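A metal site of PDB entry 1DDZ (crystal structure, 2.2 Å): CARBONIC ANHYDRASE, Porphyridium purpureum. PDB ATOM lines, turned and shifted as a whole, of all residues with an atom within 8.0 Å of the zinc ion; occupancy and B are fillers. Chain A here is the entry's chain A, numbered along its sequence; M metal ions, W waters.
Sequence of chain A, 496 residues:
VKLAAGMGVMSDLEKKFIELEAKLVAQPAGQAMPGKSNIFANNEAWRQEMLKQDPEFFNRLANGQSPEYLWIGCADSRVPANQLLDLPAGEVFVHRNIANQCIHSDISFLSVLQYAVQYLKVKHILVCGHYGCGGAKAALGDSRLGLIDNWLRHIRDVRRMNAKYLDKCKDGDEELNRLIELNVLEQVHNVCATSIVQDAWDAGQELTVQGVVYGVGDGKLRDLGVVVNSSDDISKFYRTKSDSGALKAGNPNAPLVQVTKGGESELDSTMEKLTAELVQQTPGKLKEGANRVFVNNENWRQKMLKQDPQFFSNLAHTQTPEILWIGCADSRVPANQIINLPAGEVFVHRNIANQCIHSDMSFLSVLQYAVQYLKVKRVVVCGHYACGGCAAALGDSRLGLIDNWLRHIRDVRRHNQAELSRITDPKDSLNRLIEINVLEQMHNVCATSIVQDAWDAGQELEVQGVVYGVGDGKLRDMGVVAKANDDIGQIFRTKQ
Gly 388 touches the zinc ion. Five residues have an atom within 4 Å of the zinc ion: Cys 328, Asp 330, His 384, Cys 387 and Gly 388.
The zinc ion is bound by the side-chain carboxylate (OD2) of Asp 330, a ring nitrogen (NE2) of His 384, the side-chain sulfur (SG) of Cys 387 and the side-chain sulfur (SG) of Cys 328. The zinc ion has four donor atoms within binding distance.
OD2 of Asp 330 sits close to N of Gly 388 (3.5 Å). The backbone NH of Gly 389 lies close to the side-chain sulfur of Cys 387 (3.6 Å). N of Cys 390 sits close to SG of Cys 387 (3.7 Å). The backbone NH (N) of Ala 353 lies close to the side-chain sulfur (SG) of Cys 328 (3.3 Å). The side-chain hydroxyl (OG) of Ser 331 lies within hydrogen-bond range of the backbone carbonyl oxygen (O) of Cys 328 (3.5 Å). O of Asn 351 sits close to SG of Cys 328, at 3.8 Å. The guanidinium group of Arg 350 is in hydrogen-bond range of the backbone carbonyl oxygen of Cys 328 (2.9 Å). The backbone carbonyl oxygen of Gly 388 lies close to the side-chain hydroxyl of Tyr 115.
Water W1 lies within hydrogen-bond range of OD1 of Asp 330 (3.0 Å) and N of Gly 389 (3.2 Å).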
ATOM      1  N   PHE A  93       7.729  32.263  -7.033  1.00  0.00           N
ATOM      2  CA  PHE A  93       8.337  31.597  -5.869  1.00  0.00           C
ATOM      3  C   PHE A  93       7.242  30.679  -5.310  1.00  0.00           C
ATOM      4  O   PHE A  93       6.206  31.155  -4.861  1.00  0.00           O
ATOM      5  CB  PHE A  93       8.709  32.665  -4.854  1.00  0.00           C
ATOM      6  CG  PHE A  93       9.717  32.224  -3.850  1.00  0.00           C
ATOM      7  CD1 PHE A  93      10.996  31.861  -4.252  1.00  0.00           C
ATOM      8  CD2 PHE A  93       9.403  32.200  -2.491  1.00  0.00           C
ATOM      9  CE1 PHE A  93      11.941  31.490  -3.315  1.00  0.00           C
ATOM     10  CE2 PHE A  93      10.347  31.830  -1.554  1.00  0.00           C
ATOM     11  CZ  PHE A  93      11.611  31.481  -1.963  1.00  0.00           C
ATOM     12  N   TYR A 115      10.966  35.040   3.547  1.00  0.00           N
ATOM     13  CA  TYR A 115      12.008  35.085   2.534  1.00  0.00           C
ATOM     14  C   TYR A 115      11.447  35.832   1.315  1.00  0.00           C
ATOM     15  O   TYR A 115      12.053  36.794   0.835  1.00  0.00           O
ATOM     16  CB  TYR A 115      12.437  33.666   2.134  1.00  0.00           C
ATOM     17  CG  TYR A 115      13.625  33.630   1.201  1.00  0.00           C
ATOM     18  CD1 TYR A 115      14.925  33.726   1.693  1.00  0.00           C
ATOM     19  CD2 TYR A 115      13.445  33.481  -0.177  1.00  0.00           C
ATOM     20  CE1 TYR A 115      16.038  33.668   0.841  1.00  0.00           C
ATOM     21  CE2 TYR A 115      14.540  33.432  -1.045  1.00  0.00           C
ATOM     22  CZ  TYR A 115      15.837  33.526  -0.536  1.00  0.00           C
ATOM     23  OH  TYR A 115      16.933  33.473  -1.375  1.00  0.00           O
ATOM     24  N   GLY A 327      11.479  19.836  -3.321  1.00  0.00           N
ATOM     25  CA  GLY A 327      12.383  20.803  -3.892  1.00  0.00           C
ATOM     26  C   GLY A 327      12.406  22.129  -3.196  1.00  0.00           C
ATOM     27  O   GLY A 327      11.762  22.293  -2.154  1.00  0.00           O
ATOM     28  N   CYS A 328      13.161  23.071  -3.743  1.00  0.00           N
ATOM     29  CA  CYS A 328      13.287  24.386  -3.147  1.00  0.00           C
ATOM     30  C   CYS A 328      12.270  25.374  -3.686  1.00  0.00           C
ATOM     31  O   CYS A 328      11.977  25.360  -4.877  1.00  0.00           O
ATOM     32  CB  CYS A 328      14.698  24.930  -3.388  1.00  0.00           C
ATOM     33  SG  CYS A 328      14.943  26.573  -2.621  1.00  0.00           S
ATOM     34  N   ALA A 329      11.809  26.286  -2.847  1.00  0.00           N
ATOM     35  CA  ALA A 329      10.830  27.281  -3.255  1.00  0.00           C
ATOM     36  C   ALA A 329      11.307  28.158  -4.418  1.00  0.00           C
ATOM     37  O   ALA A 329      10.500  28.813  -5.058  1.00  0.00           O
ATOM     38  CB  ALA A 329      10.376  28.094  -2.080  1.00  0.00           C
ATOM     39  N   ASP A 330      12.619  28.218  -4.650  1.00  0.00           N
ATOM     40  CA  ASP A 330      13.192  28.979  -5.755  1.00  0.00           C
ATOM     41  C   ASP A 330      12.606  28.455  -7.086  1.00  0.00           C
ATOM     42  O   ASP A 330      12.285  29.232  -7.999  1.00  0.00           O
ATOM     43  CB  ASP A 330      14.709  28.906  -5.760  1.00  0.00           C
ATOM     44  CG  ASP A 330      15.316  29.681  -4.594  1.00  0.00           C
ATOM     45  OD1 ASP A 330      14.816  30.785  -4.267  1.00  0.00           O
ATOM     46  OD2 ASP A 330      16.264  29.186  -3.968  1.00  0.00           O
ATOM     47  N   SER A 331      12.586  27.123  -7.229  1.00  0.00           N
ATOM     48  CA  SER A 331      12.001  26.439  -8.371  1.00  0.00           C
ATOM     49  C   SER A 331      12.127  27.022  -9.774  1.00  0.00           C
ATOM     50  O   SER A 331      11.132  27.441 -10.374  1.00  0.00           O
ATOM     51  CB  SER A 331      10.506  26.142  -8.087  1.00  0.00           C
ATOM     52  OG  SER A 331       9.947  27.040  -7.114  1.00  0.00           O
ATOM     53  N   ARG A 332      13.307  27.022 -10.372  1.00  0.00           N
ATOM     54  CA  ARG A 332      13.342  27.565 -11.713  1.00  0.00           C
ATOM     55  C   ARG A 332      12.869  26.563 -12.781  1.00  0.00           C
ATOM     56  O   ARG A 332      12.832  26.876 -13.974  1.00  0.00           O
ATOM     57  CB  ARG A 332      14.680  28.219 -12.066  1.00  0.00           C
ATOM     58  CG  ARG A 332      14.551  29.197 -13.244  1.00  0.00           C
ATOM     59  CD  ARG A 332      15.609  30.272 -13.201  1.00  0.00           C
ATOM     60  NE  ARG A 332      15.319  31.341 -12.236  1.00  0.00           N
ATOM     61  CZ  ARG A 332      14.663  32.485 -12.516  1.00  0.00           C
ATOM     62  NH1 ARG A 332      14.192  32.731 -13.739  1.00  0.00           N
ATOM     63  NH2 ARG A 332      14.611  33.476 -11.621  1.00  0.00           N
ATOM     64  N   ARG A 350       7.619  21.963  -1.593  1.00  0.00           N
ATOM     65  CA  ARG A 350       8.656  22.959  -1.771  1.00  0.00           C
ATOM     66  C   ARG A 350       8.727  23.863  -0.598  1.00  0.00           C
ATOM     67  O   ARG A 350       7.712  24.357  -0.116  1.00  0.00           O
ATOM     68  CB  ARG A 350       8.397  23.826  -2.980  1.00  0.00           C
ATOM     69  CG  ARG A 350       8.608  23.129  -4.262  1.00  0.00           C
ATOM     70  CD  ARG A 350       8.547  24.077  -5.409  1.00  0.00           C
ATOM     71  NE  ARG A 350       8.729  23.353  -6.660  1.00  0.00           N
ATOM     72  CZ  ARG A 350       9.890  22.849  -7.069  1.00  0.00           C
ATOM     73  NH1 ARG A 350      10.981  23.012  -6.345  1.00  0.00           N
ATOM     74  NH2 ARG A 350       9.940  22.161  -8.205  1.00  0.00           N
ATOM     75  N   ASN A 351       9.956  24.096  -0.147  1.00  0.00           N
ATOM     76  CA  ASN A 351      10.212  24.988   0.970  1.00  0.00           C
ATOM     77  C   ASN A 351      11.581  25.654   0.705  1.00  0.00           C
ATOM     78  O   ASN A 351      12.204  25.410  -0.330  1.00  0.00           O
ATOM     79  CB  ASN A 351      10.156  24.250   2.321  1.00  0.00           C
ATOM     80  CG  ASN A 351      11.226  23.187   2.465  1.00  0.00           C
ATOM     81  OD1 ASN A 351      12.287  23.261   1.852  1.00  0.00           O
ATOM     82  ND2 ASN A 351      10.950  22.186   3.271  1.00  0.00           N
ATOM     83  N   ILE A 352      12.015  26.518   1.605  1.00  0.00           N
ATOM     84  CA  ILE A 352      13.272  27.208   1.447  1.00  0.00           C
ATOM     85  C   ILE A 352      14.423  26.274   1.673  1.00  0.00           C
ATOM     86  O   ILE A 352      14.613  25.770   2.795  1.00  0.00           O
ATOM     87  CB  ILE A 352      13.416  28.379   2.454  1.00  0.00           C
ATOM     88  CG1 ILE A 352      12.412  29.470   2.120  1.00  0.00           C
ATOM     89  CG2 ILE A 352      14.813  29.013   2.343  1.00  0.00           C
ATOM     90  CD1 ILE A 352      12.520  29.941   0.697  1.00  0.00           C
ATOM     91  N   ALA A 353      15.213  26.084   0.611  1.00  0.00           N
ATOM     92  CA  ALA A 353      16.409  25.256   0.641  1.00  0.00           C
ATOM     93  C   ALA A 353      16.127  23.757   0.756  1.00  0.00           C
ATOM     94  O   ALA A 353      16.900  23.019   1.369  1.00  0.00           O
ATOM     95  CB  ALA A 353      17.321  25.709   1.762  1.00  0.00           C
ATOM     96  N   ASN A 354      15.004  23.322   0.190  1.00  0.00           N
ATOM     97  CA  ASN A 354      14.601  21.919   0.179  1.00  0.00           C
ATOM     98  C   ASN A 354      14.929  21.115   1.420  1.00  0.00           C
ATOM     99  O   ASN A 354      15.496  20.013   1.328  1.00  0.00           O
ATOM    100  CB  ASN A 354      15.110  21.205  -1.083  1.00  0.00           C
ATOM    101  CG  ASN A 354      16.563  21.548  -1.407  1.00  0.00           C
ATOM    102  OD1 ASN A 354      16.824  22.532  -2.087  1.00  0.00           O
ATOM    103  ND2 ASN A 354      17.495  20.742  -0.931  1.00  0.00           N
ATOM    104  N   CYS A 382      15.489  17.289  -4.215  1.00  0.00           N
ATOM    105  CA  CYS A 382      16.206  18.045  -5.224  1.00  0.00           C
ATOM    106  C   CYS A 382      16.681  19.411  -4.773  1.00  0.00           C
ATOM    107  O   CYS A 382      15.897  20.222  -4.278  1.00  0.00           O
ATOM    108  CB  CYS A 382      15.340  18.209  -6.465  1.00  0.00           C
ATOM    109  SG  CYS A 382      16.178  19.047  -7.847  1.00  0.00           S
ATOM    110  N   GLY A 383      17.997  19.601  -4.848  1.00  0.00           N
ATOM    111  CA  GLY A 383      18.587  20.886  -4.510  1.00  0.00           C
ATOM    112  C   GLY A 383      18.983  21.524  -5.835  1.00  0.00           C
ATOM    113  O   GLY A 383      18.836  20.892  -6.882  1.00  0.00           O
ATOM    114  N   HIS A 384      19.494  22.749  -5.840  1.00  0.00           N
ATOM    115  CA  HIS A 384      19.894  23.399  -7.096  1.00  0.00           C
ATOM    116  C   HIS A 384      21.085  24.306  -6.855  1.00  0.00           C
ATOM    117  O   HIS A 384      21.177  24.956  -5.809  1.00  0.00           O
ATOM    118  CB  HIS A 384      18.698  24.153  -7.774  1.00  0.00           C
ATOM    119  CG  HIS A 384      18.097  25.252  -6.945  1.00  0.00           C
ATOM    120  ND1 HIS A 384      18.159  26.566  -7.323  1.00  0.00           N
ATOM    121  CD2 HIS A 384      17.477  25.233  -5.741  1.00  0.00           C
ATOM    122  CE1 HIS A 384      17.614  27.318  -6.378  1.00  0.00           C
ATOM    123  NE2 HIS A 384      17.188  26.531  -5.400  1.00  0.00           N
ATOM    124  N   TYR A 385      22.003  24.361  -7.827  1.00  0.00           N
ATOM    125  CA  TYR A 385      23.199  25.188  -7.680  1.00  0.00           C
ATOM    126  C   TYR A 385      22.863  26.645  -7.540  1.00  0.00           C
ATOM    127  O   TYR A 385      21.841  27.091  -8.035  1.00  0.00           O
ATOM    128  CB  TYR A 385      24.161  24.969  -8.835  1.00  0.00           C
ATOM    129  CG  TYR A 385      24.775  23.601  -8.784  1.00  0.00           C
ATOM    130  CD1 TYR A 385      24.734  22.761  -9.886  1.00  0.00           C
ATOM    131  CD2 TYR A 385      25.358  23.132  -7.604  1.00  0.00           C
ATOM    132  CE1 TYR A 385      25.268  21.475  -9.826  1.00  0.00           C
ATOM    133  CE2 TYR A 385      25.885  21.851  -7.533  1.00  0.00           C
ATOM    134  CZ  TYR A 385      25.836  21.034  -8.653  1.00  0.00           C
ATOM    135  OH  TYR A 385      26.341  19.758  -8.580  1.00  0.00           O
ATOM    136  N   ALA A 386      23.648  27.354  -6.745  1.00  0.00           N
ATOM    137  CA  ALA A 386      23.425  28.773  -6.484  1.00  0.00           C
ATOM    138  C   ALA A 386      22.132  29.087  -5.702  1.00  0.00           C
ATOM    139  O   ALA A 386      21.721  30.236  -5.642  1.00  0.00           O
ATOM    140  CB  ALA A 386      23.489  29.584  -7.792  1.00  0.00           C
ATOM    141  N   CYS A 387      21.551  28.077  -5.054  1.00  0.00           N
ATOM    142  CA  CYS A 387      20.343  28.247  -4.229  1.00  0.00           C
ATOM    143  C   CYS A 387      20.414  29.473  -3.287  1.00  0.00           C
ATOM    144  O   CYS A 387      21.246  29.527  -2.368  1.00  0.00           O
ATOM    145  CB  CYS A 387      20.091  26.973  -3.400  1.00  0.00           C
ATOM    146  SG  CYS A 387      18.618  27.042  -2.332  1.00  0.00           S
ATOM    147  N   GLY A 388      19.485  30.412  -3.461  1.00  0.00           N
ATOM    148  CA  GLY A 388      19.438  31.619  -2.643  1.00  0.00           C
ATOM    149  C   GLY A 388      19.163  31.362  -1.180  1.00  0.00           C
ATOM    150  O   GLY A 388      19.623  32.088  -0.304  1.00  0.00           O
ATOM    151  N   GLY A 389      18.411  30.296  -0.890  1.00  0.00           N
ATOM    152  CA  GLY A 389      18.136  29.971   0.498  1.00  0.00           C
ATOM    153  C   GLY A 389      19.413  29.523   1.215  1.00  0.00           C
ATOM    154  O   GLY A 389      19.675  29.906   2.358  1.00  0.00           O
ATOM    155  N   CYS A 390      20.201  28.701   0.527  1.00  0.00           N
ATOM    156  CA  CYS A 390      21.467  28.219   1.062  1.00  0.00           C
ATOM    157  C   CYS A 390      22.469  29.347   1.170  1.00  0.00           C
ATOM    158  O   CYS A 390      23.200  29.412   2.137  1.00  0.00           O
ATOM    159  CB  CYS A 390      22.031  27.091   0.214  1.00  0.00           C
ATOM    160  SG  CYS A 390      21.077  25.566   0.387  1.00  0.00           S
ATOM    161  N   ALA A 391      22.481  30.238   0.173  1.00  0.00           N
ATOM    162  CA  ALA A 391      23.376  31.399   0.204  1.00  0.00           C
ATOM    163  C   ALA A 391      22.968  32.265   1.375  1.00  0.00           C
ATOM    164  O   ALA A 391      23.816  32.758   2.107  1.00  0.00           O
ATOM    165  CB  ALA A 391      23.239  32.182  -1.075  1.00  0.00           C
ATOM    166  N   ILE A 434      25.477  22.951  -0.886  1.00  0.00           N
ATOM    167  CA  ILE A 434      24.171  22.653  -1.474  1.00  0.00           C
ATOM    168  C   ILE A 434      24.061  21.152  -1.729  1.00  0.00           C
ATOM    169  O   ILE A 434      23.018  20.553  -1.522  1.00  0.00           O
ATOM    170  CB  ILE A 434      23.993  23.482  -2.793  1.00  0.00           C
ATOM    171  CG1 ILE A 434      23.750  24.947  -2.459  1.00  0.00           C
ATOM    172  CG2 ILE A 434      22.912  22.933  -3.678  1.00  0.00           C
ATOM    173  CD1 ILE A 434      23.536  25.775  -3.674  1.00  0.00           C
HETATM  174 ZN    ZN M   1      16.810  27.484  -3.668  1.00  0.00          ZN
HETATM  175  O   HOH W   1      15.400  29.428  -1.600  1.00  0.00           O
